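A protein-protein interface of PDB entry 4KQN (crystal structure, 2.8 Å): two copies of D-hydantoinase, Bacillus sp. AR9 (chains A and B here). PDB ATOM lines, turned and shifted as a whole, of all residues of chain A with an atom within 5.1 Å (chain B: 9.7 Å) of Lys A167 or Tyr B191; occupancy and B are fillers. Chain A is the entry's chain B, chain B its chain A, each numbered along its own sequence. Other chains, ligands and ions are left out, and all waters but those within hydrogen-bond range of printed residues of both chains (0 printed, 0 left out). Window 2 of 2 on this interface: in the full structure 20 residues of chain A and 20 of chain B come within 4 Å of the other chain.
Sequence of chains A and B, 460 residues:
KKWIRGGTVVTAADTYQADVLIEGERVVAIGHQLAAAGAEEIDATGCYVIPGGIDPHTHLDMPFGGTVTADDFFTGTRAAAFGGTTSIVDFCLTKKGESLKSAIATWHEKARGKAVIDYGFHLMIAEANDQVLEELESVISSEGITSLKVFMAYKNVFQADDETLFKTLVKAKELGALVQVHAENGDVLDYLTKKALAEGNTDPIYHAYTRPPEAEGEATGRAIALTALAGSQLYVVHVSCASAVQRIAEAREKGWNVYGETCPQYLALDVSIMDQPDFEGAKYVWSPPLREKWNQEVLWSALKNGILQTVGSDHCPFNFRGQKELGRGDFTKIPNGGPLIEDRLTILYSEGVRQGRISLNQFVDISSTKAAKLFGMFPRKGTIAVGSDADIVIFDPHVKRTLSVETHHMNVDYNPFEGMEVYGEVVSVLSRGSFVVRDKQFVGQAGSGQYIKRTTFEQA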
ATOM      1  N   ALA A 128      37.198   6.345  -6.106  1.00  0.00           N
ATOM      2  CA  ALA A 128      36.599   7.649  -6.260  1.00  0.00           C
ATOM      3  C   ALA A 128      35.595   7.857  -5.145  1.00  0.00           C
ATOM      4  O   ALA A 128      34.434   8.156  -5.379  1.00  0.00           O
ATOM      5  CB  ALA A 128      35.944   7.753  -7.612  1.00  0.00           C
ATOM      6  N   LEU A 133      37.360  12.634  -4.532  1.00  0.00           N
ATOM      7  CA  LEU A 133      36.566  13.533  -5.365  1.00  0.00           C
ATOM      8  C   LEU A 133      36.819  14.969  -4.999  1.00  0.00           C
ATOM      9  O   LEU A 133      36.633  15.865  -5.819  1.00  0.00           O
ATOM     10  CB  LEU A 133      35.075  13.245  -5.209  1.00  0.00           C
ATOM     11  CG  LEU A 133      34.402  12.166  -6.075  1.00  0.00           C
ATOM     12  CD1 LEU A 133      35.357  11.435  -7.005  1.00  0.00           C
ATOM     13  CD2 LEU A 133      33.655  11.187  -5.173  1.00  0.00           C
ATOM     14  N   ASP A 162      33.100  -0.068 -12.147  1.00  0.00           N
ATOM     15  CA  ASP A 162      32.271   0.843 -12.966  1.00  0.00           C
ATOM     16  C   ASP A 162      31.900   2.092 -12.157  1.00  0.00           C
ATOM     17  O   ASP A 162      31.858   3.185 -12.691  1.00  0.00           O
ATOM     18  CB  ASP A 162      31.006   0.135 -13.517  1.00  0.00           C
ATOM     19  CG  ASP A 162      31.308  -0.957 -14.592  1.00  0.00           C
ATOM     20  OD1 ASP A 162      32.165  -0.732 -15.480  1.00  0.00           O
ATOM     21  OD2 ASP A 162      30.649  -2.027 -14.573  1.00  0.00           O
ATOM     22  N   GLU A 163      31.677   1.913 -10.860  1.00  0.00           N
ATOM     23  CA  GLU A 163      31.376   3.006  -9.958  1.00  0.00           C
ATOM     24  C   GLU A 163      32.401   4.111 -10.014  1.00  0.00           C
ATOM     25  O   GLU A 163      32.101   5.290 -10.284  1.00  0.00           O
ATOM     26  CB  GLU A 163      31.274   2.471  -8.535  1.00  0.00           C
ATOM     27  CG  GLU A 163      31.233   3.558  -7.482  1.00  0.00           C
ATOM     28  CD  GLU A 163      30.428   3.189  -6.264  1.00  0.00           C
ATOM     29  OE1 GLU A 163      30.137   4.105  -5.481  1.00  0.00           O
ATOM     30  OE2 GLU A 163      30.051   2.013  -6.081  1.00  0.00           O
ATOM     31  N   THR A 164      33.624   3.719  -9.730  1.00  0.00           N
ATOM     32  CA  THR A 164      34.736   4.652  -9.701  1.00  0.00           C
ATOM     33  C   THR A 164      34.793   5.296 -11.063  1.00  0.00           C
ATOM     34  O   THR A 164      34.727   6.527 -11.190  1.00  0.00           O
ATOM     35  CB  THR A 164      36.028   3.892  -9.430  1.00  0.00           C
ATOM     36  OG1 THR A 164      36.002   3.391  -8.093  1.00  0.00           O
ATOM     37  CG2 THR A 164      37.209   4.770  -9.627  1.00  0.00           C
ATOM     38  N   LEU A 165      34.868   4.424 -12.083  1.00  0.00           N
ATOM     39  CA  LEU A 165      34.824   4.819 -13.498  1.00  0.00           C
ATOM     40  C   LEU A 165      33.761   5.930 -13.741  1.00  0.00           C
ATOM     41  O   LEU A 165      34.115   7.048 -14.101  1.00  0.00           O
ATOM     42  CB  LEU A 165      34.619   3.583 -14.413  1.00  0.00           C
ATOM     43  CG  LEU A 165      35.351   3.508 -15.787  1.00  0.00           C
ATOM     44  CD1 LEU A 165      34.789   2.445 -16.741  1.00  0.00           C
ATOM     45  CD2 LEU A 165      35.367   4.823 -16.532  1.00  0.00           C
ATOM     46  N   PHE A 166      32.490   5.643 -13.505  1.00  0.00           N
ATOM     47  CA  PHE A 166      31.439   6.659 -13.703  1.00  0.00           C
ATOM     48  C   PHE A 166      31.614   7.952 -12.859  1.00  0.00           C
ATOM     49  O   PHE A 166      31.626   9.073 -13.406  1.00  0.00           O
ATOM     50  CB  PHE A 166      30.051   6.046 -13.490  1.00  0.00           C
ATOM     51  CG  PHE A 166      28.916   6.906 -14.005  1.00  0.00           C
ATOM     52  CD1 PHE A 166      28.847   7.252 -15.343  1.00  0.00           C
ATOM     53  CD2 PHE A 166      27.901   7.323 -13.173  1.00  0.00           C
ATOM     54  CE1 PHE A 166      27.797   8.035 -15.832  1.00  0.00           C
ATOM     55  CE2 PHE A 166      26.853   8.089 -13.646  1.00  0.00           C
ATOM     56  CZ  PHE A 166      26.807   8.456 -14.974  1.00  0.00           C
ATOM     57  N   LYS A 167      31.755   7.811 -11.544  1.00  0.00           N
ATOM     58  CA  LYS A 167      31.941   8.990 -10.690  1.00  0.00           C
ATOM     59  C   LYS A 167      33.037   9.926 -11.217  1.00  0.00           C
ATOM     60  O   LYS A 167      32.880  11.159 -11.250  1.00  0.00           O
ATOM     61  CB  LYS A 167      32.271   8.567  -9.262  1.00  0.00           C
ATOM     62  CG  LYS A 167      31.091   7.945  -8.496  1.00  0.00           C
ATOM     63  CD  LYS A 167      31.460   7.656  -7.044  1.00  0.00           C
ATOM     64  CE  LYS A 167      30.246   7.355  -6.154  1.00  0.00           C
ATOM     65  NZ  LYS A 167      30.642   6.830  -4.809  1.00  0.00           N
ATOM     66  N   THR A 168      34.140   9.331 -11.622  1.00  0.00           N
ATOM     67  CA  THR A 168      35.285  10.064 -12.137  1.00  0.00           C
ATOM     68  C   THR A 168      34.881  10.778 -13.409  1.00  0.00           C
ATOM     69  O   THR A 168      35.248  11.928 -13.622  1.00  0.00           O
ATOM     70  CB  THR A 168      36.459   9.073 -12.396  1.00  0.00           C
ATOM     71  OG1 THR A 168      36.699   8.311 -11.212  1.00  0.00           O
ATOM     72  CG2 THR A 168      37.706   9.779 -12.799  1.00  0.00           C
ATOM     73  N   LEU A 169      34.151  10.069 -14.272  1.00  0.00           N
ATOM     74  CA  LEU A 169      33.709  10.643 -15.551  1.00  0.00           C
ATOM     75  C   LEU A 169      32.887  11.898 -15.269  1.00  0.00           C
ATOM     76  O   LEU A 169      33.120  12.928 -15.903  1.00  0.00           O
ATOM     77  CB  LEU A 169      32.849   9.676 -16.385  1.00  0.00           C
ATOM     78  CG  LEU A 169      33.351   8.738 -17.504  1.00  0.00           C
ATOM     79  CD1 LEU A 169      34.428   9.375 -18.365  1.00  0.00           C
ATOM     80  CD2 LEU A 169      33.809   7.378 -17.016  1.00  0.00           C
ATOM     81  N   VAL A 170      31.942  11.805 -14.322  1.00  0.00           N
ATOM     82  CA  VAL A 170      31.024  12.902 -14.104  1.00  0.00           C
ATOM     83  C   VAL A 170      31.759  14.056 -13.484  1.00  0.00           C
ATOM     84  O   VAL A 170      31.458  15.208 -13.775  1.00  0.00           O
ATOM     85  CB  VAL A 170      29.783  12.530 -13.261  1.00  0.00           C
ATOM     86  CG1 VAL A 170      29.096  11.304 -13.839  1.00  0.00           C
ATOM     87  CG2 VAL A 170      30.128  12.310 -11.790  1.00  0.00           C
ATOM     88  N   LYS A 171      32.700  13.757 -12.609  1.00  0.00           N
ATOM     89  CA  LYS A 171      33.536  14.807 -12.013  1.00  0.00           C
ATOM     90  C   LYS A 171      34.415  15.486 -13.099  1.00  0.00           C
ATOM     91  O   LYS A 171      34.538  16.716 -13.198  1.00  0.00           O
ATOM     92  CB  LYS A 171      34.443  14.183 -10.946  1.00  0.00           C
ATOM     93  CG  LYS A 171      34.492  14.913  -9.643  1.00  0.00           C
ATOM     94  CD  LYS A 171      34.885  16.361  -9.864  1.00  0.00           C
ATOM     95  CE  LYS A 171      34.660  17.193  -8.587  1.00  0.00           C
ATOM     96  NZ  LYS A 171      33.252  17.136  -8.080  1.00  0.00           N
ATOM     97  N   ALA A 172      35.017  14.650 -13.930  1.00  0.00           N
ATOM     98  CA  ALA A 172      35.814  15.130 -15.027  1.00  0.00           C
ATOM     99  C   ALA A 172      35.025  16.127 -15.857  1.00  0.00           C
ATOM    100  O   ALA A 172      35.510  17.171 -16.234  1.00  0.00           O
ATOM    101  CB  ALA A 172      36.242  13.945 -15.883  1.00  0.00           C
ATOM    102  N   LYS B 155      21.921  -3.316  -6.944  1.00  0.00           N
ATOM    103  CA  LYS B 155      23.173  -3.276  -6.195  1.00  0.00           C
ATOM    104  C   LYS B 155      22.915  -3.510  -4.721  1.00  0.00           C
ATOM    105  O   LYS B 155      21.918  -3.011  -4.168  1.00  0.00           O
ATOM    106  CB  LYS B 155      23.877  -1.925  -6.389  1.00  0.00           C
ATOM    107  CG  LYS B 155      25.161  -1.856  -5.595  1.00  0.00           C
ATOM    108  CD  LYS B 155      26.248  -1.014  -6.215  1.00  0.00           C
ATOM    109  CE  LYS B 155      27.569  -1.699  -5.921  1.00  0.00           C
ATOM    110  NZ  LYS B 155      28.716  -0.822  -6.231  1.00  0.00           N
ATOM    111  N   ASN B 156      23.805  -4.289  -4.103  1.00  0.00           N
ATOM    112  CA  ASN B 156      23.668  -4.718  -2.698  1.00  0.00           C
ATOM    113  C   ASN B 156      22.342  -5.417  -2.372  1.00  0.00           C
ATOM    114  O   ASN B 156      21.890  -5.342  -1.230  1.00  0.00           O
ATOM    115  CB  ASN B 156      23.837  -3.533  -1.742  1.00  0.00           C
ATOM    116  CG  ASN B 156      25.168  -2.842  -1.895  1.00  0.00           C
ATOM    117  OD1 ASN B 156      26.230  -3.461  -1.780  1.00  0.00           O
ATOM    118  ND2 ASN B 156      25.123  -1.540  -2.157  1.00  0.00           N
ATOM    119  N   GLN B 159      22.790  -8.236  -7.012  1.00  0.00           N
ATOM    120  CA  GLN B 159      23.754  -7.971  -8.084  1.00  0.00           C
ATOM    121  C   GLN B 159      25.023  -8.853  -8.091  1.00  0.00           C
ATOM    122  O   GLN B 159      25.671  -9.042  -7.060  1.00  0.00           O
ATOM    123  CB  GLN B 159      24.151  -6.505  -8.046  1.00  0.00           C
ATOM    124  CG  GLN B 159      24.955  -6.098  -9.258  1.00  0.00           C
ATOM    125  CD  GLN B 159      25.129  -4.601  -9.356  1.00  0.00           C
ATOM    126  OE1 GLN B 159      24.226  -3.835  -9.053  1.00  0.00           O
ATOM    127  NE2 GLN B 159      26.300  -4.178  -9.781  1.00  0.00           N
ATOM    128  N   ASN B 185      23.253  -1.847 -15.775  1.00  0.00           N
ATOM    129  CA  ASN B 185      24.446  -1.628 -14.993  1.00  0.00           C
ATOM    130  C   ASN B 185      24.084  -1.064 -13.642  1.00  0.00           C
ATOM    131  O   ASN B 185      24.014   0.158 -13.475  1.00  0.00           O
ATOM    132  CB  ASN B 185      25.401  -0.668 -15.703  1.00  0.00           C
ATOM    133  CG  ASN B 185      26.747  -0.605 -15.027  1.00  0.00           C
ATOM    134  OD1 ASN B 185      26.846  -0.487 -13.804  1.00  0.00           O
ATOM    135  ND2 ASN B 185      27.795  -0.697 -15.812  1.00  0.00           N
ATOM    136  N   GLY B 186      23.886  -1.964 -12.677  1.00  0.00           N
ATOM    137  CA  GLY B 186      23.744  -1.591 -11.258  1.00  0.00           C
ATOM    138  C   GLY B 186      24.549  -0.353 -10.857  1.00  0.00           C
ATOM    139  O   GLY B 186      23.995   0.638 -10.431  1.00  0.00           O
ATOM    140  N   ASP B 187      25.857  -0.374 -11.059  1.00  0.00           N
ATOM    141  CA  ASP B 187      26.693   0.711 -10.559  1.00  0.00           C
ATOM    142  C   ASP B 187      26.207   2.073 -11.038  1.00  0.00           C
ATOM    143  O   ASP B 187      26.048   2.973 -10.216  1.00  0.00           O
ATOM    144  CB  ASP B 187      28.166   0.479 -10.890  1.00  0.00           C
ATOM    145  CG  ASP B 187      28.674  -0.872 -10.363  1.00  0.00           C
ATOM    146  OD1 ASP B 187      28.776  -1.056  -9.130  1.00  0.00           O
ATOM    147  OD2 ASP B 187      28.944  -1.780 -11.188  1.00  0.00           O
ATOM    148  N   VAL B 188      25.916   2.242 -12.322  1.00  0.00           N
ATOM    149  CA  VAL B 188      25.555   3.603 -12.807  1.00  0.00           C
ATOM    150  C   VAL B 188      24.149   3.989 -12.353  1.00  0.00           C
ATOM    151  O   VAL B 188      23.852   5.168 -12.226  1.00  0.00           O
ATOM    152  CB  VAL B 188      25.692   3.845 -14.348  1.00  0.00           C
ATOM    153  CG1 VAL B 188      26.647   2.874 -15.003  1.00  0.00           C
ATOM    154  CG2 VAL B 188      24.353   3.788 -15.056  1.00  0.00           C
ATOM    155  N   LEU B 189      23.297   2.996 -12.116  1.00  0.00           N
ATOM    156  CA  LEU B 189      21.946   3.267 -11.652  1.00  0.00           C
ATOM    157  C   LEU B 189      21.957   3.743 -10.201  1.00  0.00           C
ATOM    158  O   LEU B 189      21.221   4.649  -9.817  1.00  0.00           O
ATOM    159  CB  LEU B 189      21.071   2.030 -11.780  1.00  0.00           C
ATOM    160  CG  LEU B 189      20.946   1.400 -13.158  1.00  0.00           C
ATOM    161  CD1 LEU B 189      19.743   0.482 -13.177  1.00  0.00           C
ATOM    162  CD2 LEU B 189      20.839   2.451 -14.244  1.00  0.00           C
ATOM    163  N   ASP B 190      22.805   3.120  -9.403  1.00  0.00           N
ATOM    164  CA  ASP B 190      22.895   3.487  -8.030  1.00  0.00           C
ATOM    165  C   ASP B 190      23.229   4.980  -7.956  1.00  0.00           C
ATOM    166  O   ASP B 190      22.534   5.750  -7.284  1.00  0.00           O
ATOM    167  CB  ASP B 190      23.939   2.636  -7.302  1.00  0.00           C
ATOM    168  CG  ASP B 190      23.906   2.854  -5.803  1.00  0.00           C
ATOM    169  OD1 ASP B 190      24.774   3.615  -5.329  1.00  0.00           O
ATOM    170  OD2 ASP B 190      23.003   2.304  -5.114  1.00  0.00           O
ATOM    171  N   TYR B 191      24.268   5.391  -8.673  1.00  0.00           N
ATOM    172  CA  TYR B 191      24.756   6.754  -8.541  1.00  0.00           C
ATOM    173  C   TYR B 191      23.635   7.749  -8.897  1.00  0.00           C
ATOM    174  O   TYR B 191      23.223   8.595  -8.072  1.00  0.00           O
ATOM    175  CB  TYR B 191      26.001   6.964  -9.412  1.00  0.00           C
ATOM    176  CG  TYR B 191      26.557   8.338  -9.284  1.00  0.00           C
ATOM    177  CD1 TYR B 191      27.386   8.682  -8.208  1.00  0.00           C
ATOM    178  CD2 TYR B 191      26.199   9.319 -10.198  1.00  0.00           C
ATOM    179  CE1 TYR B 191      27.867   9.965  -8.075  1.00  0.00           C
ATOM    180  CE2 TYR B 191      26.668  10.604 -10.077  1.00  0.00           C
ATOM    181  CZ  TYR B 191      27.497  10.927  -9.013  1.00  0.00           C
ATOM    182  OH  TYR B 191      27.926  12.241  -8.924  1.00  0.00           O
ATOM    183  N   LEU B 192      23.127   7.594 -10.121  1.00  0.00           N
ATOM    184  CA  LEU B 192      21.992   8.369 -10.635  1.00  0.00           C
ATOM    185  C   LEU B 192      20.800   8.354  -9.648  1.00  0.00           C
ATOM    186  O   LEU B 192      20.108   9.354  -9.475  1.00  0.00           O
ATOM    187  CB  LEU B 192      21.546   7.810 -11.993  1.00  0.00           C
ATOM    188  CG  LEU B 192      22.541   7.961 -13.152  1.00  0.00           C
ATOM    189  CD1 LEU B 192      22.182   6.983 -14.255  1.00  0.00           C
ATOM    190  CD2 LEU B 192      22.636   9.380 -13.684  1.00  0.00           C
ATOM    191  N   THR B 193      20.582   7.203  -9.025  1.00  0.00           N
ATOM    192  CA  THR B 193      19.528   7.042  -8.051  1.00  0.00           C
ATOM    193  C   THR B 193      19.817   7.872  -6.808  1.00  0.00           C
ATOM    194  O   THR B 193      18.939   8.585  -6.330  1.00  0.00           O
ATOM    195  CB  THR B 193      19.298   5.552  -7.716  1.00  0.00           C
ATOM    196  OG1 THR B 193      18.144   5.101  -8.432  1.00  0.00           O
ATOM    197  CG2 THR B 193      19.083   5.322  -6.225  1.00  0.00           C
ATOM    198  N   LYS B 194      21.037   7.794  -6.286  1.00  0.00           N
ATOM    199  CA  LYS B 194      21.366   8.521  -5.049  1.00  0.00           C
ATOM    200  C   LYS B 194      21.542  10.001  -5.306  1.00  0.00           C
ATOM    201  O   LYS B 194      21.353  10.814  -4.403  1.00  0.00           O
ATOM    202  CB  LYS B 194      22.558   7.874  -4.306  1.00  0.00           C
ATOM    203  CG  LYS B 194      22.113   6.635  -3.496  1.00  0.00           C
ATOM    204  CD  LYS B 194      23.149   5.513  -3.402  1.00  0.00           C
ATOM    205  CE  LYS B 194      24.099   5.685  -2.226  1.00  0.00           C
ATOM    206  NZ  LYS B 194      25.135   6.734  -2.502  1.00  0.00           N
ATOM    207  N   LYS B 195      21.840  10.351  -6.549  1.00  0.00           N
ATOM    208  CA  LYS B 195      21.912  11.760  -6.972  1.00  0.00           C
ATOM    209  C   LYS B 195      20.512  12.365  -7.062  1.00  0.00           C
ATOM    210  O   LYS B 195      20.279  13.479  -6.621  1.00  0.00           O
ATOM    211  CB  LYS B 195      22.603  11.870  -8.331  1.00  0.00           C
ATOM    212  CG  LYS B 195      23.150  13.226  -8.700  1.00  0.00           C
ATOM    213  CD  LYS B 195      24.280  13.048  -9.704  1.00  0.00           C
ATOM    214  CE  LYS B 195      25.311  14.173  -9.652  1.00  0.00           C
ATOM    215  NZ  LYS B 195      24.696  15.534  -9.664  1.00  0.00           N
ATOM    216  N   ALA B 196      19.589  11.642  -7.669  1.00  0.00           N
ATOM    217  CA  ALA B 196      18.255  12.169  -7.896  1.00  0.00           C
ATOM    218  C   ALA B 196      17.607  12.509  -6.578  1.00  0.00           C
ATOM    219  O   ALA B 196      16.712  13.369  -6.536  1.00  0.00           O
ATOM    220  CB  ALA B 196      17.412  11.163  -8.664  1.00  0.00           C
ATOM    221  N   LEU B 197      18.018  11.789  -5.526  1.00  0.00           N
ATOM    222  CA  LEU B 197      17.544  12.057  -4.167  1.00  0.00           C
ATOM    223  C   LEU B 197      18.254  13.276  -3.633  1.00  0.00           C
ATOM    224  O   LEU B 197      17.606  14.212  -3.181  1.00  0.00           O
ATOM    225  CB  LEU B 197      17.770  10.860  -3.231  1.00  0.00           C
ATOM    226  CG  LEU B 197      16.958   9.575  -3.498  1.00  0.00           C
ATOM    227  CD1 LEU B 197      17.170   8.478  -2.455  1.00  0.00           C
ATOM    228  CD2 LEU B 197      15.467   9.865  -3.642  1.00  0.00           C
ATOM    229  N   ALA B 198      19.580  13.289  -3.708  1.00  0.00           N
ATOM    230  CA  ALA B 198      20.347  14.490  -3.370  1.00  0.00           C
ATOM    231  C   ALA B 198      19.598  15.757  -3.753  1.00  0.00           C
ATOM    232  O   ALA B 198      19.530  16.696  -2.972  1.00  0.00           O
ATOM    233  CB  ALA B 198      21.691  14.480  -4.072  1.00  0.00           C
ATOM    234  N   GLU B 199      19.052  15.768  -4.969  1.00  0.00           N
ATOM    235  CA  GLU B 199      18.423  16.960  -5.540  1.00  0.00           C
ATOM    236  C   GLU B 199      16.933  17.123  -5.193  1.00  0.00           C
ATOM    237  O   GLU B 199      16.316  18.154  -5.475  1.00  0.00           O
ATOM    238  CB  GLU B 199      18.653  16.982  -7.056  1.00  0.00           C
ATOM    239  CG  GLU B 199      19.905  17.769  -7.453  1.00  0.00           C
ATOM    240  CD  GLU B 199      20.374  17.486  -8.884  1.00  0.00           C
ATOM    241  OE1 GLU B 199      20.083  18.330  -9.770  1.00  0.00           O
ATOM    242  OE2 GLU B 199      21.038  16.428  -9.105  1.00  0.00           O
ATOM    243  N   TYR B 209      13.968   7.943 -15.346  1.00  0.00           N
ATOM    244  CA  TYR B 209      15.146   8.733 -15.761  1.00  0.00           C
ATOM    245  C   TYR B 209      16.419   8.414 -14.962  1.00  0.00           C
ATOM    246  O   TYR B 209      17.442   8.987 -15.232  1.00  0.00           O
ATOM    247  CB  TYR B 209      14.938  10.245 -15.599  1.00  0.00           C
ATOM    248  CG  TYR B 209      13.662  10.921 -16.084  1.00  0.00           C
ATOM    249  CD1 TYR B 209      12.911  10.449 -17.145  1.00  0.00           C
ATOM    250  CD2 TYR B 209      13.270  12.101 -15.499  1.00  0.00           C
ATOM    251  CE1 TYR B 209      11.777  11.122 -17.570  1.00  0.00           C
ATOM    252  CE2 TYR B 209      12.143  12.768 -15.910  1.00  0.00           C
ATOM    253  CZ  TYR B 209      11.410  12.279 -16.945  1.00  0.00           C
ATOM    254  OH  TYR B 209      10.305  12.994 -17.311  1.00  0.00           O
ATOM    255  N   THR B 210      16.345   7.567 -13.947  1.00  0.00           N
ATOM    256  CA  THR B 210      17.539   7.148 -13.222  1.00  0.00           C
ATOM    257  C   THR B 210      18.123   5.845 -13.750  1.00  0.00           C
ATOM    258  O   THR B 210      19.052   5.275 -13.155  1.00  0.00           O
ATOM    259  CB  THR B 210      17.263   6.959 -11.724  1.00  0.00           C
ATOM    260  OG1 THR B 210      16.032   6.251 -11.542  1.00  0.00           O
ATOM    261  CG2 THR B 210      17.194   8.260 -11.094  1.00  0.00           C
ATOM    262  N   ARG B 211      17.585   5.373 -14.872  1.00  0.00           N
ATOM    263  CA  ARG B 211      18.095   4.158 -15.503  1.00  0.00           C
ATOM    264  C   ARG B 211      17.878   4.189 -17.014  1.00  0.00           C
ATOM    265  O   ARG B 211      17.139   3.367 -17.576  1.00  0.00           O
ATOM    266  CB  ARG B 211      17.457   2.956 -14.852  1.00  0.00           C
ATOM    267  CG  ARG B 211      15.964   3.085 -14.706  1.00  0.00           C
ATOM    268  CD  ARG B 211      15.493   2.314 -13.489  1.00  0.00           C
ATOM    269  NE  ARG B 211      16.023   0.968 -13.523  1.00  0.00           N
ATOM    270  CZ  ARG B 211      16.340   0.260 -12.452  1.00  0.00           C
ATOM    271  NH1 ARG B 211      16.195   0.772 -11.244  1.00  0.00           N
ATOM    272  NH2 ARG B 211      16.832  -0.958 -12.605  1.00  0.00           N
ATOM    273  N   PRO B 212      18.545   5.142 -17.668  1.00  0.00           N
ATOM    274  CA  PRO B 212      18.388   5.376 -19.082  1.00  0.00           C
ATOM    275  C   PRO B 212      18.784   4.204 -19.945  1.00  0.00           C
ATOM    276  O   PRO B 212      19.645   3.413 -19.559  1.00  0.00           O
ATOM    277  CB  PRO B 212      19.370   6.525 -19.361  1.00  0.00           C
ATOM    278  CG  PRO B 212      20.354   6.456 -18.251  1.00  0.00           C
ATOM    279  CD  PRO B 212      19.512   6.083 -17.077  1.00  0.00           C
ATOM    280  N   PHE B 331      11.242   7.009  -4.569  1.00  0.00           N
ATOM    281  CA  PHE B 331      11.022   5.866  -5.437  1.00  0.00           C
ATOM    282  C   PHE B 331      11.992   4.714  -5.213  1.00  0.00           C
ATOM    283  O   PHE B 331      11.759   3.634  -5.729  1.00  0.00           O
ATOM    284  CB  PHE B 331      11.034   6.299  -6.896  1.00  0.00           C
ATOM    285  CG  PHE B 331      12.371   6.751  -7.386  1.00  0.00           C
ATOM    286  CD1 PHE B 331      13.292   5.833  -7.899  1.00  0.00           C
ATOM    287  CD2 PHE B 331      12.707   8.097  -7.386  1.00  0.00           C
ATOM    288  CE1 PHE B 331      14.529   6.260  -8.383  1.00  0.00           C
ATOM    289  CE2 PHE B 331      13.937   8.519  -7.857  1.00  0.00           C
ATOM    290  CZ  PHE B 331      14.847   7.600  -8.357  1.00  0.00           C
ATOM    291  N   THR B 332      13.080   4.920  -4.468  1.00  0.00           N
ATOM    292  CA  THR B 332      13.962   3.783  -4.108  1.00  0.00           C
ATOM    293  C   THR B 332      13.182   2.638  -3.479  1.00  0.00           C
ATOM    294  O   THR B 332      13.504   1.483  -3.699  1.00  0.00           O
ATOM    295  CB  THR B 332      15.082   4.169  -3.120  1.00  0.00           C
ATOM    296  OG1 THR B 332      14.713   5.331  -2.362  1.00  0.00           O
ATOM    297  CG2 THR B 332      16.356   4.468  -3.878  1.00  0.00           C
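No position is printed for both chains. Of the 7 pairs that touch across the chains among the printed residues, none has its exchanged pair printed and touching as well.
ND2 of Asn B185 sits at hydrogen-bond distance from OD2 of Asp A162, 3.4 Å away. The side-chain amino group of Lys B155 is in salt-bridge range of the side-chain carboxylate of Glu A163 (3.1 Å).
OE1 of Glu A163 is in salt-bridge range of NZ of Lys A167 (2.9 Å). N of Val B188 lies within hydrogen-bond range of OD1 of Asn B185, 3.2 Å away. OE1 of Gln B159 sits close to N of Lys B155 (3.2 Å). The side-chain amino group (NZ) of Lys B155 lies within salt-bridge range of the side-chain carboxylate (OD1) of Asp B187 (2.9 Å). The side-chain amide oxygen of Asn B185 is in hydrogen-bond range of the backbone NH of Asp B187, 2.9 Å away.
Hydrophobic or aromatic side chains of chain A within 4 Å of the printed part of chain B: Phe A166 and Val A170. Hydrophobic or aromatic side chains of chain B within 4 Å of the printed part of chain A: Tyr B191. Along chain B the printed residues that touch a printed residue of chain A span positions 155 to 191. Among the printed residues, 7 pairs touch across the chains. Among the printed residues, Asp or Glu carboxylates within 4 Å of a Lys or Arg side-chain nitrogen of the other chain: Glu A163 with Lys B155.
Val A170 touches one residue of chain B. Printed residues of chain A within 4 Å of Asp B187: Asp A162 and Glu A163. Of the printed residues of chain A, Lys B155 touches Glu A163. Ala A128 touches none of the printed residues of chain B. Thr B332 touches none of the printed residues of chain A. The nearest residue of chain B that does not touch Lys A167 is Lys B194 (6.0 Å).
Among the printed residues, pairs that only touch across the chains: Val A170 with Tyr B191 (3.6 Å), Asp A162 with Asp B187 (3.7 Å), Phe A166 with Tyr B191 (3.7 Å), Lys A167 with Tyr B191 (3.8 Å) and Glu A163 with Asp B187 (3.8 Å).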
